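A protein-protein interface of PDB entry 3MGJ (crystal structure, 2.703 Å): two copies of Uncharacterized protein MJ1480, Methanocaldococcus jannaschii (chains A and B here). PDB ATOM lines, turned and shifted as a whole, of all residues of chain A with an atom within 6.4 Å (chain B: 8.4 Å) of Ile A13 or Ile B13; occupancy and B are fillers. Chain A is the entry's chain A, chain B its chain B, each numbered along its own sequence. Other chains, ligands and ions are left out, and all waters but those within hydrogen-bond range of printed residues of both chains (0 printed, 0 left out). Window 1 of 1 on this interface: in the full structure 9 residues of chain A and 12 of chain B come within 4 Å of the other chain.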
ATOM      1  N   GLY A  10      22.656 -21.037   1.913  1.00  0.00           N
ATOM      2  CA  GLY A  10      22.663 -22.038   2.960  1.00  0.00           C
ATOM      3  C   GLY A  10      21.858 -23.282   2.654  1.00  0.00           C
ATOM      4  O   GLY A  10      22.097 -23.971   1.665  1.00  0.00           O
ATOM      5  N   HIS A  11      20.906 -23.573   3.535  1.00  0.00           N
ATOM      6  CA  HIS A  11      20.075 -24.755   3.415  1.00  0.00           C
ATOM      7  C   HIS A  11      18.694 -24.465   2.905  1.00  0.00           C
ATOM      8  O   HIS A  11      17.711 -24.643   3.604  1.00  0.00           O
ATOM      9  CB  HIS A  11      20.020 -25.496   4.736  1.00  0.00           C
ATOM     10  CG  HIS A  11      21.162 -26.437   4.909  1.00  0.00           C
ATOM     11  ND1 HIS A  11      22.477 -26.020   4.853  1.00  0.00           N
ATOM     12  CD2 HIS A  11      21.199 -27.779   5.085  1.00  0.00           C
ATOM     13  CE1 HIS A  11      23.273 -27.061   5.012  1.00  0.00           C
ATOM     14  NE2 HIS A  11      22.523 -28.142   5.153  1.00  0.00           N
ATOM     15  N   ILE A  12      18.638 -24.037   1.657  1.00  0.00           N
ATOM     16  CA  ILE A  12      17.387 -23.663   1.027  1.00  0.00           C
ATOM     17  C   ILE A  12      16.365 -24.792   1.042  1.00  0.00           C
ATOM     18  O   ILE A  12      15.196 -24.569   1.340  1.00  0.00           O
ATOM     19  CB  ILE A  12      17.623 -23.211  -0.426  1.00  0.00           C
ATOM     20  CG1 ILE A  12      18.720 -22.152  -0.458  1.00  0.00           C
ATOM     21  CG2 ILE A  12      16.331 -22.674  -1.023  1.00  0.00           C
ATOM     22  CD1 ILE A  12      18.640 -21.194   0.711  1.00  0.00           C
ATOM     23  N   ILE A  13      16.823 -26.001   0.724  1.00  0.00           N
ATOM     24  CA  ILE A  13      15.968 -27.182   0.633  1.00  0.00           C
ATOM     25  C   ILE A  13      15.893 -27.951   1.950  1.00  0.00           C
ATOM     26  O   ILE A  13      16.915 -28.184   2.610  1.00  0.00           O
ATOM     27  CB  ILE A  13      16.477 -28.135  -0.465  1.00  0.00           C
ATOM     28  CG1 ILE A  13      16.665 -27.379  -1.787  1.00  0.00           C
ATOM     29  CG2 ILE A  13      15.532 -29.317  -0.632  1.00  0.00           C
ATOM     30  CD1 ILE A  13      18.043 -27.535  -2.385  1.00  0.00           C
ATOM     31  N   ASP A  14      14.675 -28.357   2.300  1.00  0.00           N
ATOM     32  CA  ASP A  14      14.351 -28.975   3.592  1.00  0.00           C
ATOM     33  C   ASP A  14      14.100 -27.865   4.614  1.00  0.00           C
ATOM     34  O   ASP A  14      13.941 -28.100   5.808  1.00  0.00           O
ATOM     35  CB  ASP A  14      15.419 -29.975   4.063  1.00  0.00           C
ATOM     36  CG  ASP A  14      14.922 -30.880   5.201  1.00  0.00           C
ATOM     37  OD1 ASP A  14      13.721 -31.252   5.204  1.00  0.00           O
ATOM     38  OD2 ASP A  14      15.734 -31.216   6.097  1.00  0.00           O
ATOM     39  N   SER A  15      14.056 -26.646   4.104  1.00  0.00           N
ATOM     40  CA  SER A  15      13.638 -25.498   4.871  1.00  0.00           C
ATOM     41  C   SER A  15      12.210 -25.150   4.455  1.00  0.00           C
ATOM     42  O   SER A  15      11.699 -25.660   3.459  1.00  0.00           O
ATOM     43  CB  SER A  15      14.567 -24.319   4.568  1.00  0.00           C
ATOM     44  OG  SER A  15      14.757 -23.505   5.711  1.00  0.00           O
ATOM     45  N   LEU A  16      11.568 -24.287   5.228  1.00  0.00           N
ATOM     46  CA  LEU A  16      10.360 -23.627   4.772  1.00  0.00           C
ATOM     47  C   LEU A  16      10.703 -22.216   4.328  1.00  0.00           C
ATOM     48  O   LEU A  16       9.810 -21.436   4.010  1.00  0.00           O
ATOM     49  CB  LEU A  16       9.325 -23.558   5.888  1.00  0.00           C
ATOM     50  CG  LEU A  16       8.711 -24.887   6.313  1.00  0.00           C
ATOM     51  CD1 LEU A  16       7.717 -24.676   7.434  1.00  0.00           C
ATOM     52  CD2 LEU A  16       8.038 -25.507   5.117  1.00  0.00           C
ATOM     53  N   ILE A  17      11.998 -21.898   4.311  1.00  0.00           N
ATOM     54  CA  ILE A  17      12.464 -20.547   4.010  1.00  0.00           C
ATOM     55  C   ILE A  17      11.866 -19.963   2.736  1.00  0.00           C
ATOM     56  O   ILE A  17      11.418 -18.818   2.726  1.00  0.00           O
ATOM     57  CB  ILE A  17      14.010 -20.460   3.901  1.00  0.00           C
ATOM     58  CG1 ILE A  17      14.451 -19.002   3.913  1.00  0.00           C
ATOM     59  CG2 ILE A  17      14.492 -21.077   2.609  1.00  0.00           C
ATOM     60  CD1 ILE A  17      13.927 -18.244   5.115  1.00  0.00           C
ATOM     61  N   LEU A  18      11.864 -20.740   1.664  1.00  0.00           N
ATOM     62  CA  LEU A  18      11.377 -20.237   0.390  1.00  0.00           C
ATOM     63  C   LEU A  18       9.911 -19.853   0.416  1.00  0.00           C
ATOM     64  O   LEU A  18       9.554 -18.762  -0.005  1.00  0.00           O
ATOM     65  CB  LEU A  18      11.596 -21.256  -0.723  1.00  0.00           C
ATOM     66  CG  LEU A  18      13.012 -21.391  -1.245  1.00  0.00           C
ATOM     67  CD1 LEU A  18      12.938 -22.233  -2.481  1.00  0.00           C
ATOM     68  CD2 LEU A  18      13.537 -20.016  -1.532  1.00  0.00           C
ATOM     69  N   PRO A  19       9.050 -20.765   0.885  1.00  0.00           N
ATOM     70  CA  PRO A  19       7.620 -20.457   0.916  1.00  0.00           C
ATOM     71  C   PRO A  19       7.348 -19.306   1.856  1.00  0.00           C
ATOM     72  O   PRO A  19       6.345 -18.611   1.712  1.00  0.00           O
ATOM     73  CB  PRO A  19       7.007 -21.731   1.483  1.00  0.00           C
ATOM     74  CG  PRO A  19       8.009 -22.797   1.199  1.00  0.00           C
ATOM     75  CD  PRO A  19       9.324 -22.141   1.328  1.00  0.00           C
ATOM     76  N   PHE A  37      19.184 -20.846  -9.243  1.00  0.00           N
ATOM     77  CA  PHE A  37      19.221 -21.752  -8.120  1.00  0.00           C
ATOM     78  C   PHE A  37      20.392 -22.703  -8.284  1.00  0.00           C
ATOM     79  O   PHE A  37      20.441 -23.455  -9.242  1.00  0.00           O
ATOM     80  CB  PHE A  37      17.922 -22.533  -8.017  1.00  0.00           C
ATOM     81  CG  PHE A  37      17.714 -23.139  -6.685  1.00  0.00           C
ATOM     82  CD1 PHE A  37      18.456 -24.234  -6.284  1.00  0.00           C
ATOM     83  CD2 PHE A  37      16.809 -22.600  -5.810  1.00  0.00           C
ATOM     84  CE1 PHE A  37      18.292 -24.799  -5.029  1.00  0.00           C
ATOM     85  CE2 PHE A  37      16.631 -23.163  -4.553  1.00  0.00           C
ATOM     86  CZ  PHE A  37      17.378 -24.273  -4.166  1.00  0.00           C
ATOM     87  N   ILE A  39      22.765 -25.723  -6.443  1.00  0.00           N
ATOM     88  CA  ILE A  39      22.993 -26.697  -5.369  1.00  0.00           C
ATOM     89  C   ILE A  39      24.482 -26.976  -5.154  1.00  0.00           C
ATOM     90  O   ILE A  39      25.264 -27.007  -6.115  1.00  0.00           O
ATOM     91  CB  ILE A  39      22.278 -28.053  -5.665  1.00  0.00           C
ATOM     92  CG1 ILE A  39      20.816 -27.998  -5.253  1.00  0.00           C
ATOM     93  CG2 ILE A  39      22.916 -29.190  -4.932  1.00  0.00           C
ATOM     94  CD1 ILE A  39      19.999 -27.141  -6.167  1.00  0.00           C
ATOM     95  N   SER A  47      23.574 -24.238  -0.679  1.00  0.00           N
ATOM     96  CA  SER A  47      23.001 -23.891  -1.975  1.00  0.00           C
ATOM     97  C   SER A  47      22.745 -22.396  -1.992  1.00  0.00           C
ATOM     98  O   SER A  47      22.889 -21.723  -0.982  1.00  0.00           O
ATOM     99  CB  SER A  47      21.692 -24.641  -2.207  1.00  0.00           C
ATOM    100  OG  SER A  47      21.811 -26.002  -1.823  1.00  0.00           O
ATOM    101  N   GLY B  10       7.401 -33.087  -7.987  1.00  0.00           N
ATOM    102  CA  GLY B  10       6.514 -33.075  -6.847  1.00  0.00           C
ATOM    103  C   GLY B  10       6.859 -32.059  -5.794  1.00  0.00           C
ATOM    104  O   GLY B  10       7.260 -30.939  -6.098  1.00  0.00           O
ATOM    105  N   HIS B  11       6.678 -32.460  -4.540  1.00  0.00           N
ATOM    106  CA  HIS B  11       7.033 -31.611  -3.412  1.00  0.00           C
ATOM    107  C   HIS B  11       8.495 -31.776  -3.029  1.00  0.00           C
ATOM    108  O   HIS B  11       8.816 -32.466  -2.067  1.00  0.00           O
ATOM    109  CB  HIS B  11       6.149 -31.887  -2.201  1.00  0.00           C
ATOM    110  CG  HIS B  11       6.491 -31.029  -1.022  1.00  0.00           C
ATOM    111  ND1 HIS B  11       6.380 -29.657  -1.050  1.00  0.00           N
ATOM    112  CD2 HIS B  11       6.972 -31.349   0.206  1.00  0.00           C
ATOM    113  CE1 HIS B  11       6.770 -29.163   0.116  1.00  0.00           C
ATOM    114  NE2 HIS B  11       7.132 -30.166   0.893  1.00  0.00           N
ATOM    115  N   ILE B  12       9.367 -31.117  -3.789  1.00  0.00           N
ATOM    116  CA  ILE B  12      10.810 -31.234  -3.623  1.00  0.00           C
ATOM    117  C   ILE B  12      11.329 -30.379  -2.481  1.00  0.00           C
ATOM    118  O   ILE B  12      12.372 -30.678  -1.904  1.00  0.00           O
ATOM    119  CB  ILE B  12      11.560 -30.770  -4.889  1.00  0.00           C
ATOM    120  CG1 ILE B  12      11.170 -31.609  -6.101  1.00  0.00           C
ATOM    121  CG2 ILE B  12      13.044 -30.877  -4.672  1.00  0.00           C
ATOM    122  CD1 ILE B  12      11.210 -33.103  -5.847  1.00  0.00           C
ATOM    123  N   ILE B  13      10.598 -29.320  -2.153  1.00  0.00           N
ATOM    124  CA  ILE B  13      11.134 -28.260  -1.302  1.00  0.00           C
ATOM    125  C   ILE B  13      11.321 -28.611   0.171  1.00  0.00           C
ATOM    126  O   ILE B  13      12.450 -28.691   0.639  1.00  0.00           O
ATOM    127  CB  ILE B  13      10.347 -26.932  -1.464  1.00  0.00           C
ATOM    128  CG1 ILE B  13      10.698 -26.282  -2.811  1.00  0.00           C
ATOM    129  CG2 ILE B  13      10.662 -25.980  -0.325  1.00  0.00           C
ATOM    130  CD1 ILE B  13      12.114 -26.554  -3.283  1.00  0.00           C
ATOM    131  N   ASP B  14      10.236 -28.813   0.907  1.00  0.00           N
ATOM    132  CA  ASP B  14      10.378 -29.079   2.336  1.00  0.00           C
ATOM    133  C   ASP B  14      10.486 -30.574   2.699  1.00  0.00           C
ATOM    134  O   ASP B  14      10.180 -30.974   3.814  1.00  0.00           O
ATOM    135  CB  ASP B  14       9.242 -28.427   3.118  1.00  0.00           C
ATOM    136  CG  ASP B  14       9.473 -28.474   4.619  1.00  0.00           C
ATOM    137  OD1 ASP B  14      10.661 -28.505   5.030  1.00  0.00           O
ATOM    138  OD2 ASP B  14       8.474 -28.490   5.380  1.00  0.00           O
ATOM    139  N   SER B  15      10.925 -31.405   1.765  1.00  0.00           N
ATOM    140  CA  SER B  15      11.060 -32.826   2.057  1.00  0.00           C
ATOM    141  C   SER B  15      12.519 -33.245   2.139  1.00  0.00           C
ATOM    142  O   SER B  15      13.417 -32.462   1.865  1.00  0.00           O
ATOM    143  CB  SER B  15      10.279 -33.698   1.053  1.00  0.00           C
ATOM    144  OG  SER B  15      10.839 -33.664  -0.234  1.00  0.00           O
ATOM    145  N   LEU B  16      12.749 -34.486   2.538  1.00  0.00           N
ATOM    146  CA  LEU B  16      14.092 -35.019   2.571  1.00  0.00           C
ATOM    147  C   LEU B  16      14.343 -35.914   1.352  1.00  0.00           C
ATOM    148  O   LEU B  16      15.325 -36.647   1.317  1.00  0.00           O
ATOM    149  CB  LEU B  16      14.304 -35.808   3.863  1.00  0.00           C
ATOM    150  CG  LEU B  16      14.104 -35.105   5.215  1.00  0.00           C
ATOM    151  CD1 LEU B  16      13.729 -36.118   6.296  1.00  0.00           C
ATOM    152  CD2 LEU B  16      15.332 -34.298   5.620  1.00  0.00           C
ATOM    153  N   ILE B  17      13.456 -35.849   0.360  1.00  0.00           N
ATOM    154  CA  ILE B  17      13.630 -36.598  -0.876  1.00  0.00           C
ATOM    155  C   ILE B  17      15.030 -36.460  -1.456  1.00  0.00           C
ATOM    156  O   ILE B  17      15.682 -37.450  -1.758  1.00  0.00           O
ATOM    157  CB  ILE B  17      12.569 -36.229  -1.959  1.00  0.00           C
ATOM    158  CG1 ILE B  17      12.777 -37.080  -3.203  1.00  0.00           C
ATOM    159  CG2 ILE B  17      12.659 -34.799  -2.379  1.00  0.00           C
ATOM    160  CD1 ILE B  17      12.610 -38.571  -2.965  1.00  0.00           C
ATOM    161  N   LEU B  18      15.495 -35.228  -1.593  1.00  0.00           N
ATOM    162  CA  LEU B  18      16.782 -34.969  -2.222  1.00  0.00           C
ATOM    163  C   LEU B  18      17.948 -35.406  -1.363  1.00  0.00           C
ATOM    164  O   LEU B  18      18.850 -36.071  -1.848  1.00  0.00           O
ATOM    165  CB  LEU B  18      16.946 -33.488  -2.571  1.00  0.00           C
ATOM    166  CG  LEU B  18      16.276 -32.967  -3.839  1.00  0.00           C
ATOM    167  CD1 LEU B  18      16.988 -31.707  -4.271  1.00  0.00           C
ATOM    168  CD2 LEU B  18      16.316 -33.997  -4.943  1.00  0.00           C
ATOM    169  N   PRO B  19      17.953 -35.010  -0.086  1.00  0.00           N
ATOM    170  CA  PRO B  19      19.090 -35.505   0.690  1.00  0.00           C
ATOM    171  C   PRO B  19      19.123 -37.028   0.663  1.00  0.00           C
ATOM    172  O   PRO B  19      20.185 -37.604   0.451  1.00  0.00           O
ATOM    173  CB  PRO B  19      18.827 -34.956   2.101  1.00  0.00           C
ATOM    174  CG  PRO B  19      17.957 -33.754   1.877  1.00  0.00           C
ATOM    175  CD  PRO B  19      17.110 -34.072   0.680  1.00  0.00           C
ATOM    176  N   PHE B  22      20.434 -38.200  -2.586  1.00  0.00           N
ATOM    177  CA  PHE B  22      21.869 -37.947  -2.687  1.00  0.00           C
ATOM    178  C   PHE B  22      22.664 -38.950  -1.869  1.00  0.00           C
ATOM    179  O   PHE B  22      23.684 -39.459  -2.331  1.00  0.00           O
ATOM    180  CB  PHE B  22      22.225 -36.518  -2.273  1.00  0.00           C
ATOM    181  CG  PHE B  22      21.677 -35.464  -3.197  1.00  0.00           C
ATOM    182  CD1 PHE B  22      21.184 -35.811  -4.446  1.00  0.00           C
ATOM    183  CD2 PHE B  22      21.660 -34.133  -2.819  1.00  0.00           C
ATOM    184  CE1 PHE B  22      20.676 -34.854  -5.300  1.00  0.00           C
ATOM    185  CE2 PHE B  22      21.162 -33.164  -3.667  1.00  0.00           C
ATOM    186  CZ  PHE B  22      20.667 -33.524  -4.913  1.00  0.00           C
ATOM    187  N   VAL B  34      23.149 -32.168 -10.213  1.00  0.00           N
ATOM    188  CA  VAL B  34      21.823 -31.609 -10.448  1.00  0.00           C
ATOM    189  C   VAL B  34      21.827 -30.673 -11.652  1.00  0.00           C
ATOM    190  O   VAL B  34      22.310 -29.546 -11.582  1.00  0.00           O
ATOM    191  CB  VAL B  34      21.314 -30.869  -9.224  1.00  0.00           C
ATOM    192  CG1 VAL B  34      19.964 -30.271  -9.508  1.00  0.00           C
ATOM    193  CG2 VAL B  34      21.264 -31.810  -8.048  1.00  0.00           C
ATOM    194  N   PHE B  37      16.826 -27.571 -11.936  1.00  0.00           N
ATOM    195  CA  PHE B  37      16.001 -27.446 -10.752  1.00  0.00           C
ATOM    196  C   PHE B  37      15.065 -26.284 -10.963  1.00  0.00           C
ATOM    197  O   PHE B  37      15.518 -25.162 -11.118  1.00  0.00           O
ATOM    198  CB  PHE B  37      16.839 -27.170  -9.519  1.00  0.00           C
ATOM    199  CG  PHE B  37      16.083 -27.346  -8.250  1.00  0.00           C
ATOM    200  CD1 PHE B  37      15.181 -26.398  -7.834  1.00  0.00           C
ATOM    201  CD2 PHE B  37      16.242 -28.481  -7.492  1.00  0.00           C
ATOM    202  CE1 PHE B  37      14.467 -26.573  -6.672  1.00  0.00           C
ATOM    203  CE2 PHE B  37      15.536 -28.655  -6.333  1.00  0.00           C
ATOM    204  CZ  PHE B  37      14.646 -27.702  -5.922  1.00  0.00           C
ATOM    205  N   GLU B  38      13.767 -26.558 -10.986  1.00  0.00           N
ATOM    206  CA  GLU B  38      12.752 -25.533 -11.135  1.00  0.00           C
ATOM    207  C   GLU B  38      11.821 -25.586  -9.939  1.00  0.00           C
ATOM    208  O   GLU B  38      11.169 -26.592  -9.716  1.00  0.00           O
ATOM    209  CB  GLU B  38      11.956 -25.760 -12.420  1.00  0.00           C
ATOM    210  CG  GLU B  38      11.247 -24.512 -12.968  1.00  0.00           C
ATOM    211  CD  GLU B  38       9.737 -24.486 -12.673  1.00  0.00           C
ATOM    212  OE1 GLU B  38       9.181 -25.536 -12.271  1.00  0.00           O
ATOM    213  OE2 GLU B  38       9.102 -23.413 -12.847  1.00  0.00           O
ATOM    214  N   ILE B  39      11.764 -24.505  -9.170  1.00  0.00           N
ATOM    215  CA  ILE B  39      10.862 -24.430  -8.031  1.00  0.00           C
ATOM    216  C   ILE B  39       9.417 -24.244  -8.465  1.00  0.00           C
ATOM    217  O   ILE B  39       9.143 -23.567  -9.448  1.00  0.00           O
ATOM    218  CB  ILE B  39      11.240 -23.275  -7.082  1.00  0.00           C
ATOM    219  CG1 ILE B  39      12.459 -23.647  -6.231  1.00  0.00           C
ATOM    220  CG2 ILE B  39      10.076 -22.922  -6.194  1.00  0.00           C
ATOM    221  CD1 ILE B  39      13.759 -23.224  -6.860  1.00  0.00           C
ATOM    222  N   GLY B  40       8.496 -24.862  -7.730  1.00  0.00           N
ATOM    223  CA  GLY B  40       7.076 -24.692  -7.983  1.00  0.00           C
ATOM    224  C   GLY B  40       6.709 -23.227  -8.137  1.00  0.00           C
ATOM    225  O   GLY B  40       6.844 -22.451  -7.191  1.00  0.00           O
ATOM    226  N   ARG B  42       4.236 -20.960  -8.092  1.00  0.00           N
ATOM    227  CA  ARG B  42       3.758 -20.379  -6.839  1.00  0.00           C
ATOM    228  C   ARG B  42       4.086 -21.374  -5.724  1.00  0.00           C
ATOM    229  O   ARG B  42       4.511 -22.502  -6.000  1.00  0.00           O
ATOM    230  CB  ARG B  42       2.250 -20.128  -6.901  1.00  0.00           C
ATOM    231  N   LYS B  43       3.916 -20.965  -4.470  1.00  0.00           N
ATOM    232  CA  LYS B  43       4.048 -21.906  -3.364  1.00  0.00           C
ATOM    233  C   LYS B  43       2.862 -22.893  -3.366  1.00  0.00           C
ATOM    234  O   LYS B  43       2.234 -23.132  -2.331  1.00  0.00           O
ATOM    235  CB  LYS B  43       4.153 -21.154  -2.033  1.00  0.00           C
ATOM    236  N   ASP B  45       2.567 -25.263  -6.684  1.00  0.00           N
ATOM    237  CA  ASP B  45       2.778 -26.198  -7.787  1.00  0.00           C
ATOM    238  C   ASP B  45       3.918 -27.213  -7.566  1.00  0.00           C
ATOM    239  O   ASP B  45       4.600 -27.190  -6.530  1.00  0.00           O
ATOM    240  CB  ASP B  45       3.002 -25.407  -9.082  1.00  0.00           C
ATOM    241  CG  ASP B  45       1.932 -24.367  -9.317  1.00  0.00           C
ATOM    242  OD1 ASP B  45       1.145 -24.524 -10.275  1.00  0.00           O
ATOM    243  OD2 ASP B  45       1.882 -23.390  -8.545  1.00  0.00           O
ATOM    244  N   PRO B  46       4.130 -28.115  -8.546  1.00  0.00           N
ATOM    245  CA  PRO B  46       5.210 -29.079  -8.348  1.00  0.00           C
ATOM    246  C   PRO B  46       6.524 -28.526  -8.875  1.00  0.00           C
ATOM    247  O   PRO B  46       6.645 -28.156 -10.054  1.00  0.00           O
ATOM    248  CB  PRO B  46       4.781 -30.260  -9.219  1.00  0.00           C
ATOM    249  CG  PRO B  46       3.915 -29.645 -10.305  1.00  0.00           C
ATOM    250  CD  PRO B  46       3.566 -28.226  -9.902  1.00  0.00           C
ATOM    251  N   SER B  47       7.507 -28.460  -7.991  1.00  0.00           N
ATOM    252  CA  SER B  47       8.867 -28.237  -8.423  1.00  0.00           C
ATOM    253  C   SER B  47       9.380 -29.524  -9.056  1.00  0.00           C
ATOM    254  O   SER B  47       8.750 -30.576  -8.955  1.00  0.00           O
ATOM    255  CB  SER B  47       9.732 -27.851  -7.228  1.00  0.00           C
ATOM    256  OG  SER B  47       9.091 -28.209  -6.014  1.00  0.00           O
ATOM    257  N   TYR B  48      10.528 -29.443  -9.710  1.00  0.00           N
ATOM    258  CA  TYR B  48      11.171 -30.648 -10.189  1.00  0.00           C
ATOM    259  C   TYR B  48      12.678 -30.503 -10.257  1.00  0.00           C
ATOM    260  O   TYR B  48      13.204 -29.408 -10.318  1.00  0.00           O
ATOM    261  CB  TYR B  48      10.610 -31.060 -11.546  1.00  0.00           C
ATOM    262  CG  TYR B  48      11.153 -30.293 -12.723  1.00  0.00           C
ATOM    263  CD1 TYR B  48      12.477 -30.464 -13.143  1.00  0.00           C
ATOM    264  CD2 TYR B  48      10.343 -29.424 -13.437  1.00  0.00           C
ATOM    265  CE1 TYR B  48      12.980 -29.784 -14.229  1.00  0.00           C
ATOM    266  CE2 TYR B  48      10.836 -28.734 -14.528  1.00  0.00           C
ATOM    267  CZ  TYR B  48      12.154 -28.916 -14.922  1.00  0.00           C
ATOM    268  OH  TYR B  48      12.653 -28.230 -16.011  1.00  0.00           O
ATOM    269  N   ALA B  49      13.367 -31.628 -10.258  1.00  0.00           N
ATOM    270  CA  ALA B  49      14.801 -31.610 -10.319  1.00  0.00           C
ATOM    271  C   ALA B  49      15.265 -32.681 -11.282  1.00  0.00           C
ATOM    272  O   ALA B  49      14.862 -33.834 -11.183  1.00  0.00           O
ATOM    273  CB  ALA B  49      15.364 -31.853  -8.938  1.00  0.00           C
ATOM    274  N   ILE B  78       6.043 -37.454  -4.255  1.00  0.00           N
ATOM    275  CA  ILE B  78       7.092 -37.269  -5.235  1.00  0.00           C
ATOM    276  C   ILE B  78       7.010 -38.347  -6.329  1.00  0.00           C
ATOM    277  O   ILE B  78       6.972 -39.555  -6.048  1.00  0.00           O
ATOM    278  CB  ILE B  78       8.496 -37.186  -4.583  1.00  0.00           C
ATOM    279  CG1 ILE B  78       9.197 -38.535  -4.602  1.00  0.00           C
ATOM    280  CG2 ILE B  78       8.401 -36.657  -3.170  1.00  0.00           C
ATOM    281  CD1 ILE B  78      10.235 -38.632  -5.673  1.00  0.00           C
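OG of Ser A15 sits close to N of Ile A17 (3.5 Å). NE2 of His B11 sits at hydrogen-bond distance from N of Asp B14, 3.4 Å away. The backbone carbonyl oxygen (O) of His B11 sits at hydrogen-bond distance from the side-chain hydroxyl (OG) of Ser B15, 3.0 Å away. The side-chain hydroxyl (OG) of Ser B15 lies close to the backbone NH (N) of Ile B17 (3.5 Å).
Ile A13 touches Ile B12, but with the chains exchanged Ile A12 does not touch Ile B13 (5.0 Å). Asp A14 touches its own counterpart, Asp B14. Ser A15 touches Ile B13, but with the chains exchanged Ile A13 does not touch Ser B15 (4.5 Å). Phe A37 touches Ile B39, but with the chains exchanged Ile A39 does not touch Phe B37 (4.2 Å). Positions printed for both chains: 10, 11, 12, 13, 14, 15, 16, 17, 18, 19, 37, 39 and 47. Of the 10 pairs that touch across the chains among the printed residues, 6 have their exchanged pair printed and touching as well.
Among the printed residues, pairs that only touch across the chains: Ile A13 with Ile B12 (3.7 Å), Ile A13 with Ile B13 (3.4 Å), Asp A14 with Ser B15 (3.6 Å), Asp A14 with Leu B16 (3.1 Å), Ser A15 with Ile B13 (3.9 Å), Leu A16 with Asp B14 (3.0 Å) and Phe A37 with Ile B39 (3.3 Å).
Of the 24 printed residues of chain B, 6 touch a printed residue of chain A. Printed residues of chain B that touch a printed residue of chain A: Ile B12, Ile B13, Asp B14, Ser B15, Leu B16 and Ile B39. Among the printed residues, 10 pairs touch across the chains. Among the printed residues, no Asp or Glu carboxylate lies within 4 Å of a Lys or Arg side-chain nitrogen of the other chain.
Printed residues of chain B within 4 Å of Ile A13: Ile B12 (3.7 Å) and Ile B13 (3.4 Å). Of the printed residues of chain B, Ser A15 touches Ile B13 and Asp B14. Of the printed residues of chain B, Phe A37 touches Ile B39. Of the printed residues of chain A, Asp B14 touches Asp A14, Ser A15 and Leu A16. Of the printed residues of chain A, Ser B15 touches Asp A14. The nearest residue of chain B that does not touch Ile A13 is Ser B15 (4.5 Å).
The backbone NH of Asp A14 sits at hydrogen-bond distance from the backbone carbonyl oxygen of Ile B13. The backbone carbonyl oxygen of Asp A14 lies close to the side-chain carboxylate of Asp B14 (3.4 Å). The backbone carbonyl oxygen (O) of Ser A15 sits close to the side-chain carboxylate (OD1) of Asp B14, 3.4 Å away.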
